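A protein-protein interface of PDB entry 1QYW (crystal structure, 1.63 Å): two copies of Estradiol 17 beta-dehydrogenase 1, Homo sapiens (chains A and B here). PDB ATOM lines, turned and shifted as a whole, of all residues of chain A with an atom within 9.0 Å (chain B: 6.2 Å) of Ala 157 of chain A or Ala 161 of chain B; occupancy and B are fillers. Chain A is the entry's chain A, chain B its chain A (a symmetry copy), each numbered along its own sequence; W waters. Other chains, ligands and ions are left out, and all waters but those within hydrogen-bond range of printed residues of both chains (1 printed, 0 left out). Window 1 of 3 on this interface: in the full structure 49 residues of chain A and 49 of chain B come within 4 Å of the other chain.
Hydrophobic or aromatic side chains of chain A within 4 Å of the printed part of chain B: Ala 157, Phe 160 and Ala 161.
Printed residues of chain B that touch a printed residue of chain A: Ala 157, Phe 160, Ala 161, Glu 163, Gly 164, Leu 165 and Ser 168.
Hydrophobic or aromatic side chains of chain B within 4 Å of the printed part of chain A: Ala 157, Phe 160, Ala 161 and Leu 165.
Among the printed residues, 13 pairs touch across the chains.
Among the printed residues, no Asp or Glu carboxylate lies within 4 Å of a Lys or Arg side-chain nitrogen of the other chain.
The backbone NH of Leu 149 of chain A is in hydrogen-bond range of the side-chain hydroxyl of Ser 168 of chain B (3.1 Å).
The side-chain sulfur of Cys 156 of chain A sits close to the side-chain hydroxyl of Ser 168 of chain B (3.5 Å).
Gly 148 of chain A touches Ser 168 of chain B (CA to OG, 3.3 Å).
Asp 153 of chain A touches Ser 168 of chain B.
Ala 161 of chain B touches Ala 157 of chain A.
Phe 160 of chain B touches Phe 160 of chain A (CB to O, 3.2 Å).
Glu 163 of chain B touches Phe 160 of chain A.
Phe 160 of chain A touches Gly 164 of chain B.
Ala 157 of chain B touches Ala 161 of chain A.
CB of Ala 161 of chain A touches CB of Ala 161 of chain B (3.99 Å).
Glu 163 of chain A touches Phe 160 of chain B.
Gly 164 of chain A touches Phe 160 of chain B.
Printed residues of chain B within 4 Å of Asp 153 of chain A: Leu 165 and Ser 168.
Ala 157 of chain A touches one residue of chain B.
Printed residues of chain A within 4 Å of Ala 157 of chain B: Ala 161 (3.3 Å).
Printed residues of chain A within 4 Å of Phe 160 of chain B: Phe 160 (3.2 Å), Glu 163 (3.9 Å) and Gly 164 (3.4 Å).
Of the printed residues of chain A, Ala 161 of chain B touches Ala 157 (3.3 Å) and Ala 161 (3.99 Å).
Of chain A, only Phe 160 comes within 4 Å of Gly 164 of chain B.
Cys 166 of chain B touches none of the printed residues of chain A.
The nearest residue of chain B that does not touch Ala 157 of chain A is Leu 165 of chain B (4.2 Å).
The nearest printed residue of chain B that does not touch Gly 164 of chain A is Cys 156 of chain B (4.1 Å).
O of Gly 144 of chain A lies within hydrogen-bond range of SG of Cys 156 of chain A.
SG of Cys 156 of chain A sits close to O of Asn 152 of chain A, at 3.3 Å.
The backbone carbonyl oxygen of Gly 164 of chain B lies within hydrogen-bond range of the side-chain hydroxyl of Ser 168 of chain B (2.8 Å).
N of Leu 149 of chain A lies within hydrogen-bond range of SG of Cys 156 of chain A (3.4 Å).
Ala 157 of chain A touches Ala 161 of chain B, and with the chains exchanged Ala 161 of chain A touches Ala 157 of chain B.
Phe 160 of chain A touches Glu 163 of chain B, and with the chains exchanged Glu 163 of chain A touches Phe 160 of chain B.
Phe 160 of chain A touches Gly 164 of chain B, and with the chains exchanged Gly 164 of chain A touches Phe 160 of chain B.
Ala 161 of chain A touches its own counterpart, Ala 161 of chain B.
13 positions are printed for both chains.
Of the 13 pairs that touch across the chains among the printed residues, 8 have their exchanged pair printed and touching as well.
Water W1 bridges the side-chain carboxylate of Asp 153 of chain A (2.6 Å) and the backbone carbonyl oxygen of Ser 168 of chain B (3.1 Å).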
ATOM      1  N   LEU A  95       5.070 -32.335   5.175  1.00  0.00           N
ATOM      2  CA  LEU A  95       3.728 -32.489   5.701  1.00  0.00           C
ATOM      3  C   LEU A  95       2.865 -32.985   4.540  1.00  0.00           C
ATOM      4  O   LEU A  95       2.776 -32.276   3.518  1.00  0.00           O
ATOM      5  CB  LEU A  95       3.180 -31.175   6.277  1.00  0.00           C
ATOM      6  CG  LEU A  95       1.849 -31.326   7.019  1.00  0.00           C
ATOM      7  CD1 LEU A  95       1.875 -32.366   8.119  1.00  0.00           C
ATOM      8  CD2 LEU A  95       1.437 -29.954   7.588  1.00  0.00           C
ATOM      9  N   LEU A  99      -5.610 -31.310   3.122  1.00  0.00           N
ATOM     10  CA  LEU A  99      -5.491 -30.094   3.929  1.00  0.00           C
ATOM     11  C   LEU A  99      -6.364 -30.096   5.172  1.00  0.00           C
ATOM     12  O   LEU A  99      -5.883 -29.803   6.264  1.00  0.00           O
ATOM     13  CB  LEU A  99      -5.860 -28.852   3.082  1.00  0.00           C
ATOM     14  CG  LEU A  99      -5.575 -27.554   3.872  1.00  0.00           C
ATOM     15  CD1 LEU A  99      -4.099 -27.216   3.899  1.00  0.00           C
ATOM     16  CD2 LEU A  99      -6.460 -26.442   3.309  1.00  0.00           C
ATOM     17  N   VAL A 107       0.609 -27.679  10.909  1.00  0.00           N
ATOM     18  CA  VAL A 107       0.789 -26.602   9.903  1.00  0.00           C
ATOM     19  C   VAL A 107       1.690 -25.483  10.391  1.00  0.00           C
ATOM     20  O   VAL A 107       2.646 -25.062   9.736  1.00  0.00           O
ATOM     21  CB  VAL A 107      -0.605 -26.023   9.511  1.00  0.00           C
ATOM     22  CG1 VAL A 107      -0.443 -24.829   8.575  1.00  0.00           C
ATOM     23  CG2 VAL A 107      -1.403 -27.158   8.885  1.00  0.00           C
ATOM     24  N   VAL A 110       5.330 -26.585  10.514  1.00  0.00           N
ATOM     25  CA  VAL A 110       6.040 -26.651   9.223  1.00  0.00           C
ATOM     26  C   VAL A 110       6.508 -25.255   8.818  1.00  0.00           C
ATOM     27  O   VAL A 110       7.683 -25.088   8.464  1.00  0.00           O
ATOM     28  CB  VAL A 110       5.121 -27.223   8.123  1.00  0.00           C
ATOM     29  CG1 VAL A 110       5.609 -26.854   6.724  1.00  0.00           C
ATOM     30  CG2 VAL A 110       4.981 -28.718   8.339  1.00  0.00           C
ATOM     31  N   LEU A 111       5.609 -24.270   8.940  1.00  0.00           N
ATOM     32  CA  LEU A 111       6.024 -22.894   8.612  1.00  0.00           C
ATOM     33  C   LEU A 111       7.052 -22.343   9.587  1.00  0.00           C
ATOM     34  O   LEU A 111       7.948 -21.649   9.116  1.00  0.00           O
ATOM     35  CB  LEU A 111       4.787 -21.997   8.553  1.00  0.00           C
ATOM     36  CG  LEU A 111       3.922 -22.030   7.290  1.00  0.00           C
ATOM     37  CD1 LEU A 111       4.742 -22.194   6.010  1.00  0.00           C
ATOM     38  CD2 LEU A 111       2.838 -23.080   7.333  1.00  0.00           C
ATOM     39  N   ASN A 114      10.478 -24.391   8.646  1.00  0.00           N
ATOM     40  CA  ASN A 114      10.945 -24.244   7.264  1.00  0.00           C
ATOM     41  C   ASN A 114      11.211 -22.788   6.887  1.00  0.00           C
ATOM     42  O   ASN A 114      12.188 -22.481   6.195  1.00  0.00           O
ATOM     43  CB  ASN A 114       9.985 -24.877   6.254  1.00  0.00           C
ATOM     44  CG  ASN A 114       9.948 -26.409   6.382  1.00  0.00           C
ATOM     45  OD1 ASN A 114      10.673 -26.958   7.209  1.00  0.00           O
ATOM     46  ND2 ASN A 114       9.119 -27.007   5.544  1.00  0.00           N
ATOM     47  N   VAL A 115      10.318 -21.899   7.272  1.00  0.00           N
ATOM     48  CA  VAL A 115      10.401 -20.489   6.897  1.00  0.00           C
ATOM     49  C   VAL A 115      10.925 -19.616   8.032  1.00  0.00           C
ATOM     50  O   VAL A 115      11.981 -19.038   7.812  1.00  0.00           O
ATOM     51  CB  VAL A 115       9.016 -19.936   6.440  1.00  0.00           C
ATOM     52  CG1 VAL A 115       9.179 -18.580   5.793  1.00  0.00           C
ATOM     53  CG2 VAL A 115       8.424 -20.960   5.468  1.00  0.00           C
ATOM     54  N   GLY A 144       8.957 -28.813  -5.152  1.00  0.00           N
ATOM     55  CA  GLY A 144       7.698 -28.386  -4.539  1.00  0.00           C
ATOM     56  C   GLY A 144       7.673 -26.904  -4.144  1.00  0.00           C
ATOM     57  O   GLY A 144       6.626 -26.393  -3.692  1.00  0.00           O
ATOM     58  N   GLY A 145       8.806 -26.206  -4.244  1.00  0.00           N
ATOM     59  CA  GLY A 145       8.852 -24.753  -4.014  1.00  0.00           C
ATOM     60  C   GLY A 145       8.667 -24.036  -5.364  1.00  0.00           C
ATOM     61  O   GLY A 145       8.582 -22.812  -5.383  1.00  0.00           O
ATOM     62  N   LEU A 146       8.682 -24.826  -6.453  1.00  0.00           N
ATOM     63  CA  LEU A 146       8.592 -24.215  -7.792  1.00  0.00           C
ATOM     64  C   LEU A 146       7.265 -24.500  -8.508  1.00  0.00           C
ATOM     65  O   LEU A 146       6.851 -23.790  -9.449  1.00  0.00           O
ATOM     66  CB  LEU A 146       9.740 -24.799  -8.648  1.00  0.00           C
ATOM     67  CG  LEU A 146      11.160 -24.616  -8.087  1.00  0.00           C
ATOM     68  CD1 LEU A 146      12.178 -25.199  -9.081  1.00  0.00           C
ATOM     69  CD2 LEU A 146      11.438 -23.128  -7.899  1.00  0.00           C
ATOM     70  N   MET A 147       6.580 -25.517  -8.030  1.00  0.00           N
ATOM     71  CA  MET A 147       5.278 -25.933  -8.553  1.00  0.00           C
ATOM     72  C   MET A 147       4.485 -26.637  -7.492  1.00  0.00           C
ATOM     73  O   MET A 147       4.977 -27.372  -6.615  1.00  0.00           O
ATOM     74  CB  MET A 147       5.497 -26.798  -9.803  1.00  0.00           C
ATOM     75  CG  MET A 147       6.140 -28.134  -9.429  1.00  0.00           C
ATOM     76  SD  MET A 147       6.573 -29.003 -10.965  1.00  0.00           S
ATOM     77  CE  MET A 147       7.967 -28.077 -11.502  1.00  0.00           C
ATOM     78  N   GLY A 148       3.167 -26.359  -7.450  1.00  0.00           N
ATOM     79  CA  GLY A 148       2.288 -26.939  -6.452  1.00  0.00           C
ATOM     80  C   GLY A 148       1.994 -28.424  -6.617  1.00  0.00           C
ATOM     81  O   GLY A 148       1.778 -28.861  -7.747  1.00  0.00           O
ATOM     82  N   LEU A 149       2.098 -29.168  -5.521  1.00  0.00           N
ATOM     83  CA  LEU A 149       1.881 -30.623  -5.557  1.00  0.00           C
ATOM     84  C   LEU A 149       0.689 -30.991  -4.708  1.00  0.00           C
ATOM     85  O   LEU A 149       0.573 -30.616  -3.531  1.00  0.00           O
ATOM     86  CB  LEU A 149       3.154 -31.315  -5.075  1.00  0.00           C
ATOM     87  CG  LEU A 149       4.472 -30.866  -5.727  1.00  0.00           C
ATOM     88  CD1 LEU A 149       5.625 -31.474  -4.955  1.00  0.00           C
ATOM     89  CD2 LEU A 149       4.415 -31.240  -7.190  1.00  0.00           C
ATOM     90  N   ASN A 152       0.366 -31.824  -0.668  1.00  0.00           N
ATOM     91  CA  ASN A 152       1.575 -31.225  -0.129  1.00  0.00           C
ATOM     92  C   ASN A 152       1.326 -29.707  -0.005  1.00  0.00           C
ATOM     93  O   ASN A 152       2.288 -28.928  -0.093  1.00  0.00           O
ATOM     94  CB  ASN A 152       2.737 -31.398  -1.107  1.00  0.00           C
ATOM     95  CG  ASN A 152       3.299 -32.805  -1.089  1.00  0.00           C
ATOM     96  OD1 ASN A 152       4.275 -33.149  -0.398  1.00  0.00           O
ATOM     97  ND2 ASN A 152       2.666 -33.682  -1.882  1.00  0.00           N
ATOM     98  N   ASP A 153       0.119 -29.284   0.233  1.00  0.00           N
ATOM     99  CA  ASP A 153      -0.285 -27.867   0.211  1.00  0.00           C
ATOM    100  C   ASP A 153       0.535 -27.018   1.151  1.00  0.00           C
ATOM    101  O   ASP A 153       1.094 -25.973   0.745  1.00  0.00           O
ATOM    102  CB  ASP A 153      -1.777 -27.740   0.569  1.00  0.00           C
ATOM    103  CG  ASP A 153      -2.634 -28.695  -0.236  1.00  0.00           C
ATOM    104  OD1 ASP A 153      -2.875 -28.513  -1.438  1.00  0.00           O
ATOM    105  OD2 ASP A 153      -3.116 -29.693   0.325  1.00  0.00           O
ATOM    106  N   VAL A 154       0.644 -27.481   2.400  1.00  0.00           N
ATOM    107  CA  VAL A 154       1.413 -26.651   3.366  1.00  0.00           C
ATOM    108  C   VAL A 154       2.889 -26.831   3.160  1.00  0.00           C
ATOM    109  O   VAL A 154       3.674 -25.870   3.259  1.00  0.00           O
ATOM    110  CB  VAL A 154       0.948 -26.927   4.800  1.00  0.00           C
ATOM    111  CG1 VAL A 154       1.819 -26.148   5.784  1.00  0.00           C
ATOM    112  CG2 VAL A 154      -0.524 -26.603   4.957  1.00  0.00           C
ATOM    113  N   TYR A 155       3.395 -28.013   2.769  1.00  0.00           N
ATOM    114  CA  TYR A 155       4.791 -28.217   2.474  1.00  0.00           C
ATOM    115  C   TYR A 155       5.214 -27.316   1.293  1.00  0.00           C
ATOM    116  O   TYR A 155       6.205 -26.579   1.371  1.00  0.00           O
ATOM    117  CB  TYR A 155       5.095 -29.654   2.054  1.00  0.00           C
ATOM    118  CG  TYR A 155       6.516 -29.893   1.610  1.00  0.00           C
ATOM    119  CD1 TYR A 155       7.583 -29.900   2.484  1.00  0.00           C
ATOM    120  CD2 TYR A 155       6.769 -30.048   0.255  1.00  0.00           C
ATOM    121  CE1 TYR A 155       8.863 -30.122   2.023  1.00  0.00           C
ATOM    122  CE2 TYR A 155       8.036 -30.256  -0.245  1.00  0.00           C
ATOM    123  CZ  TYR A 155       9.078 -30.304   0.671  1.00  0.00           C
ATOM    124  OH  TYR A 155      10.358 -30.510   0.216  1.00  0.00           O
ATOM    125  N   CYS A 156       4.417 -27.370   0.225  1.00  0.00           N
ATOM    126  CA  CYS A 156       4.718 -26.469  -0.929  1.00  0.00           C
ATOM    127  C   CYS A 156       4.584 -25.019  -0.459  1.00  0.00           C
ATOM    128  O   CYS A 156       5.385 -24.164  -0.892  1.00  0.00           O
ATOM    129  CB  CYS A 156       3.670 -26.693  -2.038  1.00  0.00           C
ATOM    130  SG  CYS A 156       4.011 -28.315  -2.836  1.00  0.00           S
ATOM    131  N   ALA A 157       3.609 -24.665   0.392  1.00  0.00           N
ATOM    132  CA  ALA A 157       3.528 -23.247   0.835  1.00  0.00           C
ATOM    133  C   ALA A 157       4.880 -22.869   1.419  1.00  0.00           C
ATOM    134  O   ALA A 157       5.459 -21.783   1.164  1.00  0.00           O
ATOM    135  CB  ALA A 157       2.449 -23.053   1.902  1.00  0.00           C
ATOM    136  N   SER A 158       5.401 -23.726   2.286  1.00  0.00           N
ATOM    137  CA  SER A 158       6.681 -23.403   2.941  1.00  0.00           C
ATOM    138  C   SER A 158       7.854 -23.283   2.013  1.00  0.00           C
ATOM    139  O   SER A 158       8.792 -22.471   2.140  1.00  0.00           O
ATOM    140  CB  SER A 158       6.899 -24.434   4.081  1.00  0.00           C
ATOM    141  OG  SER A 158       7.471 -25.603   3.576  1.00  0.00           O
ATOM    142  N   LYS A 159       7.934 -24.154   0.958  1.00  0.00           N
ATOM    143  CA  LYS A 159       9.060 -24.163   0.044  1.00  0.00           C
ATOM    144  C   LYS A 159       8.933 -22.978  -0.937  1.00  0.00           C
ATOM    145  O   LYS A 159       9.937 -22.350  -1.286  1.00  0.00           O
ATOM    146  CB  LYS A 159       9.203 -25.499  -0.693  1.00  0.00           C
ATOM    147  CG  LYS A 159       9.409 -26.674   0.292  1.00  0.00           C
ATOM    148  CD  LYS A 159      10.619 -26.547   1.171  1.00  0.00           C
ATOM    149  CE  LYS A 159      11.939 -26.370   0.448  1.00  0.00           C
ATOM    150  NZ  LYS A 159      13.057 -27.025   1.250  1.00  0.00           N
ATOM    151  N   PHE A 160       7.729 -22.655  -1.369  1.00  0.00           N
ATOM    152  CA  PHE A 160       7.463 -21.475  -2.183  1.00  0.00           C
ATOM    153  C   PHE A 160       7.921 -20.254  -1.342  1.00  0.00           C
ATOM    154  O   PHE A 160       8.536 -19.297  -1.822  1.00  0.00           O
ATOM    155  CB  PHE A 160       5.975 -21.283  -2.518  1.00  0.00           C
ATOM    156  CG  PHE A 160       5.524 -21.947  -3.797  1.00  0.00           C
ATOM    157  CD1 PHE A 160       5.535 -23.310  -3.961  1.00  0.00           C
ATOM    158  CD2 PHE A 160       5.019 -21.136  -4.805  1.00  0.00           C
ATOM    159  CE1 PHE A 160       5.096 -23.870  -5.166  1.00  0.00           C
ATOM    160  CE2 PHE A 160       4.594 -21.709  -5.999  1.00  0.00           C
ATOM    161  CZ  PHE A 160       4.609 -23.063  -6.191  1.00  0.00           C
ATOM    162  N   ALA A 161       7.562 -20.299  -0.045  1.00  0.00           N
ATOM    163  CA  ALA A 161       7.985 -19.163   0.833  1.00  0.00           C
ATOM    164  C   ALA A 161       9.488 -18.959   0.786  1.00  0.00           C
ATOM    165  O   ALA A 161       9.902 -17.778   0.710  1.00  0.00           O
ATOM    166  CB  ALA A 161       7.475 -19.376   2.259  1.00  0.00           C
ATOM    167  N   LEU A 162      10.287 -20.040   0.842  1.00  0.00           N
ATOM    168  CA  LEU A 162      11.745 -19.882   0.794  1.00  0.00           C
ATOM    169  C   LEU A 162      12.163 -19.259  -0.508  1.00  0.00           C
ATOM    170  O   LEU A 162      13.135 -18.485  -0.544  1.00  0.00           O
ATOM    171  CB  LEU A 162      12.463 -21.247   1.000  1.00  0.00           C
ATOM    172  CG  LEU A 162      12.474 -21.760   2.438  1.00  0.00           C
ATOM    173  CD1 LEU A 162      13.130 -23.148   2.491  1.00  0.00           C
ATOM    174  CD2 LEU A 162      13.240 -20.798   3.332  1.00  0.00           C
ATOM    175  N   GLU A 163      11.495 -19.608  -1.628  1.00  0.00           N
ATOM    176  CA  GLU A 163      11.825 -18.979  -2.898  1.00  0.00           C
ATOM    177  C   GLU A 163      11.650 -17.447  -2.790  1.00  0.00           C
ATOM    178  O   GLU A 163      12.540 -16.686  -3.202  1.00  0.00           O
ATOM    179  CB  GLU A 163      10.935 -19.484  -4.038  1.00  0.00           C
ATOM    180  CG  GLU A 163      11.141 -20.982  -4.305  1.00  0.00           C
ATOM    181  CD  GLU A 163      12.455 -21.294  -5.027  1.00  0.00           C
ATOM    182  OE1 GLU A 163      12.817 -20.619  -6.002  1.00  0.00           O
ATOM    183  OE2 GLU A 163      13.139 -22.272  -4.620  1.00  0.00           O
ATOM    184  N   GLY A 164      10.508 -17.010  -2.278  1.00  0.00           N
ATOM    185  CA  GLY A 164      10.242 -15.575  -2.187  1.00  0.00           C
ATOM    186  C   GLY A 164      11.238 -14.900  -1.246  1.00  0.00           C
ATOM    187  O   GLY A 164      11.781 -13.832  -1.519  1.00  0.00           O
ATOM    188  N   LEU A 165      11.495 -15.552  -0.100  1.00  0.00           N
ATOM    189  CA  LEU A 165      12.430 -15.011   0.866  1.00  0.00           C
ATOM    190  C   LEU A 165      13.810 -14.820   0.252  1.00  0.00           C
ATOM    191  O   LEU A 165      14.428 -13.727   0.328  1.00  0.00           O
ATOM    192  CB  LEU A 165      12.543 -16.028   2.029  1.00  0.00           C
ATOM    193  CG  LEU A 165      13.630 -15.642   3.066  1.00  0.00           C
ATOM    194  CD1 LEU A 165      13.285 -14.327   3.719  1.00  0.00           C
ATOM    195  CD2 LEU A 165      13.744 -16.718   4.145  1.00  0.00           C
ATOM    196  N   LEU B 111       3.430 -14.443   8.793  1.00  0.00           N
ATOM    197  CA  LEU B 111       3.130 -15.806   8.317  1.00  0.00           C
ATOM    198  C   LEU B 111       1.873 -16.384   8.947  1.00  0.00           C
ATOM    199  O   LEU B 111       1.147 -17.057   8.223  1.00  0.00           O
ATOM    200  CB  LEU B 111       4.338 -16.706   8.577  1.00  0.00           C
ATOM    201  CG  LEU B 111       5.522 -16.636   7.608  1.00  0.00           C
ATOM    202  CD1 LEU B 111       5.092 -16.426   6.156  1.00  0.00           C
ATOM    203  CD2 LEU B 111       6.546 -15.593   7.986  1.00  0.00           C
ATOM    204  N   VAL B 115      -0.614 -16.736   5.799  1.00  0.00           N
ATOM    205  CA  VAL B 115      -0.582 -18.133   5.370  1.00  0.00           C
ATOM    206  C   VAL B 115      -1.398 -19.041   6.284  1.00  0.00           C
ATOM    207  O   VAL B 115      -2.348 -19.606   5.759  1.00  0.00           O
ATOM    208  CB  VAL B 115       0.878 -18.678   5.300  1.00  0.00           C
ATOM    209  CG1 VAL B 115       0.909 -20.011   4.589  1.00  0.00           C
ATOM    210  CG2 VAL B 115       1.713 -17.625   4.566  1.00  0.00           C
ATOM    211  N   GLY B 145       4.036 -12.063  -4.688  1.00  0.00           N
ATOM    212  CA  GLY B 145       3.935 -13.523  -4.528  1.00  0.00           C
ATOM    213  C   GLY B 145       4.493 -14.196  -5.795  1.00  0.00           C
ATOM    214  O   GLY B 145       4.586 -15.420  -5.830  1.00  0.00           O
ATOM    215  N   CYS B 156       6.996 -11.066   0.864  1.00  0.00           N
ATOM    216  CA  CYS B 156       7.034 -11.928  -0.357  1.00  0.00           C
ATOM    217  C   CYS B 156       7.038 -13.393   0.085  1.00  0.00           C
ATOM    218  O   CYS B 156       6.394 -14.230  -0.583  1.00  0.00           O
ATOM    219  CB  CYS B 156       8.349 -11.672  -1.121  1.00  0.00           C
ATOM    220  SG  CYS B 156       8.237 -10.023  -1.929  1.00  0.00           S
ATOM    221  N   ALA B 157       7.737 -13.779   1.162  1.00  0.00           N
ATOM    222  CA  ALA B 157       7.698 -15.211   1.563  1.00  0.00           C
ATOM    223  C   ALA B 157       6.239 -15.601   1.733  1.00  0.00           C
ATOM    224  O   ALA B 157       5.759 -16.676   1.292  1.00  0.00           O
ATOM    225  CB  ALA B 157       8.437 -15.444   2.883  1.00  0.00           C
ATOM    226  N   SER B 158       5.492 -14.771   2.448  1.00  0.00           N
ATOM    227  CA  SER B 158       4.081 -15.109   2.708  1.00  0.00           C
ATOM    228  C   SER B 158       3.215 -15.193   1.486  1.00  0.00           C
ATOM    229  O   SER B 158       2.283 -16.004   1.319  1.00  0.00           O
ATOM    230  CB  SER B 158       3.549 -14.114   3.775  1.00  0.00           C
ATOM    231  OG  SER B 158       3.135 -12.927   3.169  1.00  0.00           O
ATOM    232  N   LYS B 159       3.429 -14.287   0.480  1.00  0.00           N
ATOM    233  CA  LYS B 159       2.603 -14.244  -0.712  1.00  0.00           C
ATOM    234  C   LYS B 159       3.006 -15.397  -1.656  1.00  0.00           C
ATOM    235  O   LYS B 159       2.142 -16.008  -2.292  1.00  0.00           O
ATOM    236  CB  LYS B 159       2.666 -12.883  -1.415  1.00  0.00           C
ATOM    237  CG  LYS B 159       2.187 -11.740  -0.489  1.00  0.00           C
ATOM    238  CD  LYS B 159       0.781 -11.891   0.012  1.00  0.00           C
ATOM    239  CE  LYS B 159      -0.283 -12.038  -1.057  1.00  0.00           C
ATOM    240  NZ  LYS B 159      -1.585 -11.404  -0.578  1.00  0.00           N
ATOM    241  N   PHE B 160       4.284 -15.711  -1.745  1.00  0.00           N
ATOM    242  CA  PHE B 160       4.772 -16.865  -2.490  1.00  0.00           C
ATOM    243  C   PHE B 160       4.102 -18.111  -1.851  1.00  0.00           C
ATOM    244  O   PHE B 160       3.651 -19.048  -2.515  1.00  0.00           O
ATOM    245  CB  PHE B 160       6.295 -17.053  -2.401  1.00  0.00           C
ATOM    246  CG  PHE B 160       7.083 -16.349  -3.482  1.00  0.00           C
ATOM    247  CD1 PHE B 160       7.112 -14.982  -3.597  1.00  0.00           C
ATOM    248  CD2 PHE B 160       7.853 -17.129  -4.335  1.00  0.00           C
ATOM    249  CE1 PHE B 160       7.868 -14.385  -4.613  1.00  0.00           C
ATOM    250  CE2 PHE B 160       8.592 -16.520  -5.342  1.00  0.00           C
ATOM    251  CZ  PHE B 160       8.625 -15.161  -5.487  1.00  0.00           C
ATOM    252  N   ALA B 161       4.085 -18.110  -0.505  1.00  0.00           N
ATOM    253  CA  ALA B 161       3.439 -19.272   0.183  1.00  0.00           C
ATOM    254  C   ALA B 161       2.009 -19.467  -0.289  1.00  0.00           C
ATOM    255  O   ALA B 161       1.639 -20.643  -0.516  1.00  0.00           O
ATOM    256  CB  ALA B 161       3.529 -19.108   1.701  1.00  0.00           C
ATOM    257  N   LEU B 162       1.222 -18.384  -0.423  1.00  0.00           N
ATOM    258  CA  LEU B 162      -0.163 -18.534  -0.882  1.00  0.00           C
ATOM    259  C   LEU B 162      -0.199 -19.112  -2.269  1.00  0.00           C
ATOM    260  O   LEU B 162      -1.119 -19.881  -2.600  1.00  0.00           O
ATOM    261  CB  LEU B 162      -0.917 -17.173  -0.841  1.00  0.00           C
ATOM    262  CG  LEU B 162      -1.333 -16.707   0.553  1.00  0.00           C
ATOM    263  CD1 LEU B 162      -1.983 -15.319   0.466  1.00  0.00           C
ATOM    264  CD2 LEU B 162      -2.313 -17.695   1.166  1.00  0.00           C
ATOM    265  N   GLU B 163       0.754 -18.731  -3.145  1.00  0.00           N
ATOM    266  CA  GLU B 163       0.796 -19.316  -4.476  1.00  0.00           C
ATOM    267  C   GLU B 163       0.940 -20.852  -4.374  1.00  0.00           C
ATOM    268  O   GLU B 163       0.204 -21.594  -5.043  1.00  0.00           O
ATOM    269  CB  GLU B 163       1.966 -18.779  -5.305  1.00  0.00           C
ATOM    270  CG  GLU B 163       1.836 -17.272  -5.570  1.00  0.00           C
ATOM    271  CD  GLU B 163       0.775 -16.930  -6.621  1.00  0.00           C
ATOM    272  OE1 GLU B 163       0.703 -17.571  -7.679  1.00  0.00           O
ATOM    273  OE2 GLU B 163       0.000 -15.963  -6.389  1.00  0.00           O
ATOM    274  N   GLY B 164       1.896 -21.310  -3.578  1.00  0.00           N
ATOM    275  CA  GLY B 164       2.132 -22.748  -3.463  1.00  0.00           C
ATOM    276  C   GLY B 164       0.916 -23.449  -2.860  1.00  0.00           C
ATOM    277  O   GLY B 164       0.476 -24.505  -3.309  1.00  0.00           O
ATOM    278  N   LEU B 165       0.346 -22.834  -1.812  1.00  0.00           N
ATOM    279  CA  LEU B 165      -0.819 -23.402  -1.163  1.00  0.00           C
ATOM    280  C   LEU B 165      -1.972 -23.566  -2.144  1.00  0.00           C
ATOM    281  O   LEU B 165      -2.582 -24.659  -2.280  1.00  0.00           O
ATOM    282  CB  LEU B 165      -1.257 -22.423  -0.045  1.00  0.00           C
ATOM    283  CG  LEU B 165      -2.588 -22.837   0.633  1.00  0.00           C
ATOM    284  CD1 LEU B 165      -2.434 -24.175   1.314  1.00  0.00           C
ATOM    285  CD2 LEU B 165      -3.005 -21.797   1.672  1.00  0.00           C
ATOM    286  N   CYS B 166      -2.308 -22.503  -2.857  1.00  0.00           N
ATOM    287  CA  CYS B 166      -3.443 -22.486  -3.751  1.00  0.00           C
ATOM    288  C   CYS B 166      -3.271 -23.362  -4.967  1.00  0.00           C
ATOM    289  O   CYS B 166      -4.180 -24.091  -5.357  1.00  0.00           O
ATOM    290  CB  CYS B 166      -3.731 -21.033  -4.230  1.00  0.00           C
ATOM    291  SG  CYS B 166      -4.461 -20.123  -2.842  1.00  0.00           S
ATOM    292  N   SER B 168      -1.346 -26.028  -5.204  1.00  0.00           N
ATOM    293  CA  SER B 168      -1.405 -27.400  -4.711  1.00  0.00           C
ATOM    294  C   SER B 168      -2.841 -27.853  -4.536  1.00  0.00           C
ATOM    295  O   SER B 168      -3.240 -28.923  -5.038  1.00  0.00           O
ATOM    296  CB  SER B 168      -0.638 -27.579  -3.378  1.00  0.00           C
ATOM    297  OG  SER B 168       0.729 -27.253  -3.562  1.00  0.00           O
HETATM  298  O   HOH W   1      -3.807 -30.644  -2.544  1.00  0.00           O
